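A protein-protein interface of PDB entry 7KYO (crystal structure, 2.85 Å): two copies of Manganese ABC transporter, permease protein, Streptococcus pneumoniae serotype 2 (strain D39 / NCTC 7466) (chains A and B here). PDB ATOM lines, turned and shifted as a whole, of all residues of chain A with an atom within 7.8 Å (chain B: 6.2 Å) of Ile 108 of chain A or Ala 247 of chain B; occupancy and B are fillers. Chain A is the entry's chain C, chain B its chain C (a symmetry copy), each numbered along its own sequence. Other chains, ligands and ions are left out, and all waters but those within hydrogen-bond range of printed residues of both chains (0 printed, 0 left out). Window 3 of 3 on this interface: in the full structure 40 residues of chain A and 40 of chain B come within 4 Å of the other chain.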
ATOM      1  N   LEU A  53      21.238 -13.392  -6.562  1.00  0.00           N
ATOM      2  CA  LEU A  53      20.084 -12.541  -6.885  1.00  0.00           C
ATOM      3  C   LEU A  53      20.430 -11.319  -7.758  1.00  0.00           C
ATOM      4  O   LEU A  53      19.683 -11.015  -8.689  1.00  0.00           O
ATOM      5  CB  LEU A  53      19.329 -12.128  -5.608  1.00  0.00           C
ATOM      6  CG  LEU A  53      18.059 -11.283  -5.765  1.00  0.00           C
ATOM      7  CD1 LEU A  53      16.991 -12.041  -6.540  1.00  0.00           C
ATOM      8  CD2 LEU A  53      17.529 -10.866  -4.403  1.00  0.00           C
ATOM      9  N   PRO A  54      21.543 -10.614  -7.459  1.00  0.00           N
ATOM     10  CA  PRO A  54      22.044  -9.607  -8.403  1.00  0.00           C
ATOM     11  C   PRO A  54      22.297 -10.148  -9.813  1.00  0.00           C
ATOM     12  O   PRO A  54      21.911  -9.510 -10.788  1.00  0.00           O
ATOM     13  CB  PRO A  54      23.361  -9.168  -7.768  1.00  0.00           C
ATOM     14  CG  PRO A  54      23.120  -9.306  -6.314  1.00  0.00           C
ATOM     15  CD  PRO A  54      22.209 -10.491  -6.148  1.00  0.00           C
ATOM     16  N   ALA A  57      19.100 -10.676 -11.489  1.00  0.00           N
ATOM     17  CA  ALA A  57      18.542  -9.343 -11.756  1.00  0.00           C
ATOM     18  C   ALA A  57      19.143  -8.673 -12.997  1.00  0.00           C
ATOM     19  O   ALA A  57      18.401  -8.141 -13.823  1.00  0.00           O
ATOM     20  CB  ALA A  57      18.704  -8.439 -10.539  1.00  0.00           C
ATOM     21  N   SER A 101      23.751 -10.375   2.656  1.00  0.00           N
ATOM     22  CA  SER A 101      22.679  -9.407   2.926  1.00  0.00           C
ATOM     23  C   SER A 101      22.769  -8.155   2.053  1.00  0.00           C
ATOM     24  O   SER A 101      21.744  -7.631   1.617  1.00  0.00           O
ATOM     25  CB  SER A 101      22.684  -9.000   4.402  1.00  0.00           C
ATOM     26  OG  SER A 101      22.500 -10.127   5.239  1.00  0.00           O
ATOM     27  N   SER A 102      23.993  -7.682   1.812  1.00  0.00           N
ATOM     28  CA  SER A 102      24.238  -6.538   0.923  1.00  0.00           C
ATOM     29  C   SER A 102      23.884  -6.851  -0.537  1.00  0.00           C
ATOM     30  O   SER A 102      23.306  -6.011  -1.228  1.00  0.00           O
ATOM     31  CB  SER A 102      25.698  -6.084   1.026  1.00  0.00           C
ATOM     32  OG  SER A 102      25.948  -4.949   0.218  1.00  0.00           O
ATOM     33  N   PHE A 103      24.238  -8.053  -0.996  1.00  0.00           N
ATOM     34  CA  PHE A 103      23.865  -8.522  -2.340  1.00  0.00           C
ATOM     35  C   PHE A 103      22.351  -8.725  -2.475  1.00  0.00           C
ATOM     36  O   PHE A 103      21.790  -8.470  -3.539  1.00  0.00           O
ATOM     37  CB  PHE A 103      24.604  -9.821  -2.707  1.00  0.00           C
ATOM     38  CG  PHE A 103      25.987  -9.608  -3.277  1.00  0.00           C
ATOM     39  CD1 PHE A 103      26.866  -8.670  -2.731  1.00  0.00           C
ATOM     40  CD2 PHE A 103      26.420 -10.363  -4.363  1.00  0.00           C
ATOM     41  CE1 PHE A 103      28.135  -8.492  -3.263  1.00  0.00           C
ATOM     42  CE2 PHE A 103      27.686 -10.185  -4.898  1.00  0.00           C
ATOM     43  CZ  PHE A 103      28.546  -9.249  -4.348  1.00  0.00           C
ATOM     44  N   LEU A 104      21.700  -9.187  -1.406  1.00  0.00           N
ATOM     45  CA  LEU A 104      20.232  -9.301  -1.373  1.00  0.00           C
ATOM     46  C   LEU A 104      19.565  -7.931  -1.508  1.00  0.00           C
ATOM     47  O   LEU A 104      18.632  -7.770  -2.295  1.00  0.00           O
ATOM     48  CB  LEU A 104      19.767  -9.985  -0.081  1.00  0.00           C
ATOM     49  CG  LEU A 104      18.260 -10.075   0.204  1.00  0.00           C
ATOM     50  CD1 LEU A 104      17.532 -10.763  -0.943  1.00  0.00           C
ATOM     51  CD2 LEU A 104      18.005 -10.771   1.539  1.00  0.00           C
ATOM     52  N   ALA A 105      20.047  -6.960  -0.733  1.00  0.00           N
ATOM     53  CA  ALA A 105      19.574  -5.573  -0.813  1.00  0.00           C
ATOM     54  C   ALA A 105      19.836  -4.951  -2.187  1.00  0.00           C
ATOM     55  O   ALA A 105      19.004  -4.197  -2.696  1.00  0.00           O
ATOM     56  CB  ALA A 105      20.221  -4.727   0.274  1.00  0.00           C
ATOM     57  N   LEU A 106      20.994  -5.267  -2.768  1.00  0.00           N
ATOM     58  CA  LEU A 106      21.338  -4.840  -4.129  1.00  0.00           C
ATOM     59  C   LEU A 106      20.354  -5.425  -5.142  1.00  0.00           C
ATOM     60  O   LEU A 106      19.897  -4.721  -6.040  1.00  0.00           O
ATOM     61  CB  LEU A 106      22.779  -5.246  -4.479  1.00  0.00           C
ATOM     62  CG  LEU A 106      23.427  -4.636  -5.737  1.00  0.00           C
ATOM     63  CD1 LEU A 106      24.947  -4.602  -5.601  1.00  0.00           C
ATOM     64  CD2 LEU A 106      23.022  -5.353  -7.023  1.00  0.00           C
ATOM     65  N   GLY A 107      20.024  -6.706  -4.981  1.00  0.00           N
ATOM     66  CA  GLY A 107      19.059  -7.387  -5.846  1.00  0.00           C
ATOM     67  C   GLY A 107      17.643  -6.827  -5.816  1.00  0.00           C
ATOM     68  O   GLY A 107      16.957  -6.837  -6.839  1.00  0.00           O
ATOM     69  N   ILE A 108      17.208  -6.337  -4.655  1.00  0.00           N
ATOM     70  CA  ILE A 108      15.845  -5.812  -4.482  1.00  0.00           C
ATOM     71  C   ILE A 108      15.652  -4.463  -5.191  1.00  0.00           C
ATOM     72  O   ILE A 108      14.681  -4.295  -5.932  1.00  0.00           O
ATOM     73  CB  ILE A 108      15.457  -5.706  -2.984  1.00  0.00           C
ATOM     74  CG1 ILE A 108      15.372  -7.106  -2.361  1.00  0.00           C
ATOM     75  CG2 ILE A 108      14.120  -4.987  -2.799  1.00  0.00           C
ATOM     76  CD1 ILE A 108      15.542  -7.125  -0.856  1.00  0.00           C
ATOM     77  N   ILE A 109      16.560  -3.512  -4.959  1.00  0.00           N
ATOM     78  CA  ILE A 109      16.446  -2.174  -5.573  1.00  0.00           C
ATOM     79  C   ILE A 109      16.721  -2.190  -7.081  1.00  0.00           C
ATOM     80  O   ILE A 109      16.147  -1.389  -7.822  1.00  0.00           O
ATOM     81  CB  ILE A 109      17.329  -1.097  -4.873  1.00  0.00           C
ATOM     82  CG1 ILE A 109      18.835  -1.313  -5.129  1.00  0.00           C
ATOM     83  CG2 ILE A 109      17.028  -1.041  -3.380  1.00  0.00           C
ATOM     84  CD1 ILE A 109      19.419  -0.470  -6.250  1.00  0.00           C
ATOM     85  N   LEU A 110      17.587  -3.103  -7.522  1.00  0.00           N
ATOM     86  CA  LEU A 110      17.944  -3.226  -8.941  1.00  0.00           C
ATOM     87  C   LEU A 110      16.787  -3.784  -9.785  1.00  0.00           C
ATOM     88  O   LEU A 110      16.605  -3.371 -10.931  1.00  0.00           O
ATOM     89  CB  LEU A 110      19.198  -4.093  -9.107  1.00  0.00           C
ATOM     90  CG  LEU A 110      19.957  -3.990 -10.429  1.00  0.00           C
ATOM     91  CD1 LEU A 110      20.588  -2.614 -10.605  1.00  0.00           C
ATOM     92  CD2 LEU A 110      21.023  -5.070 -10.485  1.00  0.00           C
ATOM     93  N   ILE A 111      16.020  -4.717  -9.219  1.00  0.00           N
ATOM     94  CA  ILE A 111      14.776  -5.194  -9.843  1.00  0.00           C
ATOM     95  C   ILE A 111      13.666  -4.141  -9.713  1.00  0.00           C
ATOM     96  O   ILE A 111      12.906  -3.931 -10.660  1.00  0.00           O
ATOM     97  CB  ILE A 111      14.310  -6.549  -9.245  1.00  0.00           C
ATOM     98  CG1 ILE A 111      15.329  -7.646  -9.576  1.00  0.00           C
ATOM     99  CG2 ILE A 111      12.935  -6.952  -9.778  1.00  0.00           C
ATOM    100  CD1 ILE A 111      15.142  -8.931  -8.796  1.00  0.00           C
ATOM    101  N   GLY A 112      13.580  -3.492  -8.549  1.00  0.00           N
ATOM    102  CA  GLY A 112      12.544  -2.491  -8.269  1.00  0.00           C
ATOM    103  C   GLY A 112      12.507  -1.299  -9.214  1.00  0.00           C
ATOM    104  O   GLY A 112      11.434  -0.908  -9.680  1.00  0.00           O
ATOM    105  N   VAL A 113      13.677  -0.721  -9.489  1.00  0.00           N
ATOM    106  CA  VAL A 113      13.786   0.434 -10.402  1.00  0.00           C
ATOM    107  C   VAL A 113      13.554   0.090 -11.881  1.00  0.00           C
ATOM    108  O   VAL A 113      12.863   0.832 -12.587  1.00  0.00           O
ATOM    109  CB  VAL A 113      15.132   1.203 -10.253  1.00  0.00           C
ATOM    110  CG1 VAL A 113      15.277   1.760  -8.841  1.00  0.00           C
ATOM    111  CG2 VAL A 113      16.342   0.355 -10.651  1.00  0.00           C
ATOM    112  N   ALA A 114      14.118  -1.029 -12.339  1.00  0.00           N
ATOM    113  CA  ALA A 114      14.048  -1.426 -13.749  1.00  0.00           C
ATOM    114  C   ALA A 114      12.721  -2.105 -14.080  1.00  0.00           C
ATOM    115  O   ALA A 114      11.983  -1.645 -14.954  1.00  0.00           O
ATOM    116  CB  ALA A 114      15.211  -2.345 -14.101  1.00  0.00           C
ATOM    117  N   LYS A 115      12.431  -3.194 -13.370  1.00  0.00           N
ATOM    118  CA  LYS A 115      11.231  -4.007 -13.604  1.00  0.00           C
ATOM    119  C   LYS A 115      10.100  -3.642 -12.638  1.00  0.00           C
ATOM    120  O   LYS A 115      10.290  -2.847 -11.713  1.00  0.00           O
ATOM    121  CB  LYS A 115      11.578  -5.499 -13.501  1.00  0.00           C
ATOM    122  CG  LYS A 115      12.455  -6.009 -14.635  1.00  0.00           C
ATOM    123  CD  LYS A 115      11.668  -6.183 -15.926  1.00  0.00           C
ATOM    124  CE  LYS A 115      12.554  -6.664 -17.064  1.00  0.00           C
ATOM    125  NZ  LYS A 115      11.813  -6.729 -18.353  1.00  0.00           N
ATOM    126  N   SER A 116       8.925  -4.227 -12.870  1.00  0.00           N
ATOM    127  CA  SER A 116       7.707  -3.891 -12.122  1.00  0.00           C
ATOM    128  C   SER A 116       7.694  -4.440 -10.688  1.00  0.00           C
ATOM    129  O   SER A 116       8.608  -5.157 -10.274  1.00  0.00           O
ATOM    130  CB  SER A 116       6.471  -4.388 -12.885  1.00  0.00           C
ATOM    131  OG  SER A 116       5.285  -3.808 -12.370  1.00  0.00           O
ATOM    132  N   LEU A 120       9.237  -8.645  -8.605  1.00  0.00           N
ATOM    133  CA  LEU A 120      10.012  -8.925  -7.386  1.00  0.00           C
ATOM    134  C   LEU A 120       9.468 -10.125  -6.602  1.00  0.00           C
ATOM    135  O   LEU A 120      10.241 -10.887  -6.018  1.00  0.00           O
ATOM    136  CB  LEU A 120      10.039  -7.689  -6.474  1.00  0.00           C
ATOM    137  CG  LEU A 120      10.902  -7.740  -5.205  1.00  0.00           C
ATOM    138  CD1 LEU A 120      12.377  -7.859  -5.557  1.00  0.00           C
ATOM    139  CD2 LEU A 120      10.653  -6.511  -4.344  1.00  0.00           C
ATOM    140  N   LEU A 124      11.766 -13.801  -5.523  1.00  0.00           N
ATOM    141  CA  LEU A 124      12.048 -14.055  -4.105  1.00  0.00           C
ATOM    142  C   LEU A 124      11.212 -15.198  -3.505  1.00  0.00           C
ATOM    143  O   LEU A 124      11.671 -15.877  -2.582  1.00  0.00           O
ATOM    144  CB  LEU A 124      11.868 -12.771  -3.286  1.00  0.00           C
ATOM    145  CG  LEU A 124      12.763 -11.584  -3.673  1.00  0.00           C
ATOM    146  CD1 LEU A 124      12.399 -10.346  -2.867  1.00  0.00           C
ATOM    147  CD2 LEU A 124      14.238 -11.915  -3.494  1.00  0.00           C
ATOM    148  N   ILE A 199      14.267 -17.035  -1.067  1.00  0.00           N
ATOM    149  CA  ILE A 199      14.160 -16.966   0.395  1.00  0.00           C
ATOM    150  C   ILE A 199      14.074 -18.364   1.020  1.00  0.00           C
ATOM    151  O   ILE A 199      14.829 -18.673   1.942  1.00  0.00           O
ATOM    152  CB  ILE A 199      12.959 -16.090   0.833  1.00  0.00           C
ATOM    153  CG1 ILE A 199      13.174 -14.638   0.384  1.00  0.00           C
ATOM    154  CG2 ILE A 199      12.756 -16.142   2.346  1.00  0.00           C
ATOM    155  CD1 ILE A 199      11.905 -13.817   0.318  1.00  0.00           C
ATOM    156  N   PHE B 125       9.470  -7.173   4.625  1.00  0.00           N
ATOM    157  CA  PHE B 125      10.309  -6.022   4.245  1.00  0.00           C
ATOM    158  C   PHE B 125       9.916  -4.799   5.083  1.00  0.00           C
ATOM    159  O   PHE B 125       9.042  -4.897   5.947  1.00  0.00           O
ATOM    160  CB  PHE B 125      10.171  -5.739   2.747  1.00  0.00           C
ATOM    161  CG  PHE B 125      10.499  -6.922   1.879  1.00  0.00           C
ATOM    162  CD1 PHE B 125      11.824  -7.269   1.627  1.00  0.00           C
ATOM    163  CD2 PHE B 125       9.487  -7.700   1.323  1.00  0.00           C
ATOM    164  CE1 PHE B 125      12.134  -8.364   0.831  1.00  0.00           C
ATOM    165  CE2 PHE B 125       9.791  -8.796   0.526  1.00  0.00           C
ATOM    166  CZ  PHE B 125      11.115  -9.128   0.279  1.00  0.00           C
ATOM    167  N   ILE B 199      13.573 -10.170   6.589  1.00  0.00           N
ATOM    168  CA  ILE B 199      14.544 -10.717   5.634  1.00  0.00           C
ATOM    169  C   ILE B 199      15.907 -10.027   5.760  1.00  0.00           C
ATOM    170  O   ILE B 199      16.930 -10.702   5.881  1.00  0.00           O
ATOM    171  CB  ILE B 199      14.014 -10.635   4.180  1.00  0.00           C
ATOM    172  CG1 ILE B 199      12.767 -11.516   4.023  1.00  0.00           C
ATOM    173  CG2 ILE B 199      15.082 -11.062   3.175  1.00  0.00           C
ATOM    174  CD1 ILE B 199      11.901 -11.154   2.835  1.00  0.00           C
ATOM    175  N   LEU B 200      15.910  -8.695   5.746  1.00  0.00           N
ATOM    176  CA  LEU B 200      17.151  -7.903   5.801  1.00  0.00           C
ATOM    177  C   LEU B 200      17.558  -7.438   7.217  1.00  0.00           C
ATOM    178  O   LEU B 200      18.464  -6.613   7.366  1.00  0.00           O
ATOM    179  CB  LEU B 200      17.027  -6.700   4.858  1.00  0.00           C
ATOM    180  CG  LEU B 200      17.025  -7.015   3.360  1.00  0.00           C
ATOM    181  CD1 LEU B 200      16.514  -5.817   2.575  1.00  0.00           C
ATOM    182  CD2 LEU B 200      18.411  -7.421   2.876  1.00  0.00           C
ATOM    183  N   GLY B 237      19.289   6.202   4.414  1.00  0.00           N
ATOM    184  CA  GLY B 237      18.491   5.203   3.703  1.00  0.00           C
ATOM    185  C   GLY B 237      17.016   5.551   3.559  1.00  0.00           C
ATOM    186  O   GLY B 237      16.380   5.159   2.581  1.00  0.00           O
ATOM    187  N   GLY B 241      15.486   6.417  -0.017  1.00  0.00           N
ATOM    188  CA  GLY B 241      14.325   5.572  -0.304  1.00  0.00           C
ATOM    189  C   GLY B 241      13.066   6.351  -0.653  1.00  0.00           C
ATOM    190  O   GLY B 241      12.333   5.971  -1.570  1.00  0.00           O
ATOM    191  N   ASN B 245      12.007   6.933  -4.651  1.00  0.00           N
ATOM    192  CA  ASN B 245      10.888   5.982  -4.691  1.00  0.00           C
ATOM    193  C   ASN B 245      11.382   4.559  -4.974  1.00  0.00           C
ATOM    194  O   ASN B 245      11.138   3.987  -6.041  1.00  0.00           O
ATOM    195  CB  ASN B 245       9.800   6.431  -5.685  1.00  0.00           C
ATOM    196  CG  ASN B 245       8.515   5.629  -5.553  1.00  0.00           C
ATOM    197  OD1 ASN B 245       8.039   5.038  -6.523  1.00  0.00           O
ATOM    198  ND2 ASN B 245       7.950   5.600  -4.351  1.00  0.00           N
ATOM    199  N   VAL B 246      12.102   4.017  -3.995  1.00  0.00           N
ATOM    200  CA  VAL B 246      12.629   2.650  -4.033  1.00  0.00           C
ATOM    201  C   VAL B 246      12.395   1.996  -2.672  1.00  0.00           C
ATOM    202  O   VAL B 246      11.901   2.648  -1.746  1.00  0.00           O
ATOM    203  CB  VAL B 246      14.133   2.622  -4.411  1.00  0.00           C
ATOM    204  CG1 VAL B 246      14.324   3.052  -5.858  1.00  0.00           C
ATOM    205  CG2 VAL B 246      14.972   3.501  -3.485  1.00  0.00           C
ATOM    206  N   ALA B 247      12.737   0.713  -2.561  1.00  0.00           N
ATOM    207  CA  ALA B 247      12.595  -0.037  -1.306  1.00  0.00           C
ATOM    208  C   ALA B 247      13.356   0.636  -0.159  1.00  0.00           C
ATOM    209  O   ALA B 247      14.553   0.906  -0.279  1.00  0.00           O
ATOM    210  CB  ALA B 247      13.077  -1.470  -1.486  1.00  0.00           C
ATOM    211  N   ALA B 248      12.648   0.907   0.938  1.00  0.00           N
ATOM    212  CA  ALA B 248      13.210   1.634   2.079  1.00  0.00           C
ATOM    213  C   ALA B 248      14.238   0.796   2.832  1.00  0.00           C
ATOM    214  O   ALA B 248      15.349   1.260   3.087  1.00  0.00           O
ATOM    215  CB  ALA B 248      12.104   2.084   3.024  1.00  0.00           C
ATOM    216  N   GLY B 249      13.862  -0.436   3.172  1.00  0.00           N
ATOM    217  CA  GLY B 249      14.733  -1.354   3.906  1.00  0.00           C
ATOM    218  C   GLY B 249      16.031  -1.689   3.192  1.00  0.00           C
ATOM    219  O   GLY B 249      17.102  -1.629   3.792  1.00  0.00           O
ATOM    220  N   SER B 250      15.936  -2.029   1.907  1.00  0.00           N
ATOM    221  CA  SER B 250      17.110  -2.395   1.101  1.00  0.00           C
ATOM    222  C   SER B 250      18.109  -1.244   0.927  1.00  0.00           C
ATOM    223  O   SER B 250      19.318  -1.475   0.885  1.00  0.00           O
ATOM    224  CB  SER B 250      16.676  -2.917  -0.271  1.00  0.00           C
ATOM    225  OG  SER B 250      15.800  -4.021  -0.133  1.00  0.00           O
ATOM    226  N   SER B 251      17.602  -0.017   0.827  1.00  0.00           N
ATOM    227  CA  SER B 251      18.449   1.180   0.759  1.00  0.00           C
ATOM    228  C   SER B 251      19.210   1.433   2.064  1.00  0.00           C
ATOM    229  O   SER B 251      20.368   1.856   2.041  1.00  0.00           O
ATOM    230  CB  SER B 251      17.604   2.404   0.422  1.00  0.00           C
ATOM    231  OG  SER B 251      16.926   2.224  -0.806  1.00  0.00           O
ATOM    232  N   ILE B 252      18.548   1.173   3.190  1.00  0.00           N
ATOM    233  CA  ILE B 252      19.153   1.307   4.520  1.00  0.00           C
ATOM    234  C   ILE B 252      20.297   0.292   4.712  1.00  0.00           C
ATOM    235  O   ILE B 252      21.309   0.610   5.342  1.00  0.00           O
ATOM    236  CB  ILE B 252      18.078   1.175   5.637  1.00  0.00           C
ATOM    237  CG1 ILE B 252      17.101   2.360   5.579  1.00  0.00           C
ATOM    238  CG2 ILE B 252      18.709   1.095   7.026  1.00  0.00           C
ATOM    239  CD1 ILE B 252      15.799   2.134   6.320  1.00  0.00           C
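Of the 22 printed residues of chain A, 8 touch a printed residue of chain B.
Printed residues of chain A that touch a printed residue of chain B: Ser 101, Leu 104, Ala 105, Ile 108, Ile 109, Val 113, Leu 124 and Ile 199.
Hydrophobic or aromatic side chains of chain A within 4 Å of the printed part of chain B: Leu 104, Ala 105, Ile 108, Ile 109, Val 113, Leu 124 and Ile 199.
Of the 13 printed residues of chain B, 6 touch a printed residue of chain A.
Printed residues of chain B that touch a printed residue of chain A: Phe 125, Ile 199, Leu 200, Val 246, Ala 247 and Ser 250.
Hydrophobic or aromatic side chains of chain B within 4 Å of the printed part of chain A: Phe 125, Ile 199, Leu 200, Val 246 and Ala 247.
Ala 247 of chain B touches just one residue of chain A: Ile 108 (3.9 Å).
Printed residues of chain A within 4 Å of Ile 199 of chain B: Leu 104 (3.4 Å) and Ile 199 (3.7 Å).
Of the printed residues of chain B, Ser 101 of chain A touches Leu 200 (3.6 Å).
Printed residues of chain B within 4 Å of Leu 104 of chain A: Ile 199 and Leu 200.
Of the printed residues of chain A, Val 246 of chain B touches Val 113 (3.4 Å).
The nearest residue of chain A that does not touch Ala 247 of chain B is Ile 109 of chain A (4.4 Å).
Ile 199 of chain A touches its own counterpart, Ile 199 of chain B.
Leu 200 of chain B touches Ser 101 of chain A.
Leu 104 of chain A touches Ile 199 of chain B (CD2 to CG2, 3.4 Å).
CD2 of Leu 200 of chain B touches N of Ala 105 of chain A, at 3.99 Å.
O of Ser 250 of chain B touches CB of Ala 105 of chain A (3.4 Å).
CE1 of Phe 125 of chain B touches CD1 of Ile 108 of chain A, at 3.999 Å.
CD1 of Ile 108 of chain A touches CD1 of Leu 200 of chain B, at 3.8 Å.
Ser 250 of chain B touches Ile 108 of chain A.
Val 113 of chain A touches Val 246 of chain B (CG1 to CG1, 3.4 Å).
CD1 of Leu 124 of chain A touches CZ of Phe 125 of chain B, 3.6 Å away.
CD1 of Ile 199 of chain B touches CD1 of Ile 199 of chain A (3.7 Å).
N of Ile 199 of chain A is in hydrogen-bond range of O of Leu 124 of chain A, 3.2 Å away.
The backbone NH (N) of Val 246 of chain B sits at hydrogen-bond distance from the backbone carbonyl oxygen (O) of Gly 241 of chain B.
O of Ala 247 of chain B is in hydrogen-bond range of OG of Ser 251 of chain B, at 2.8 Å.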
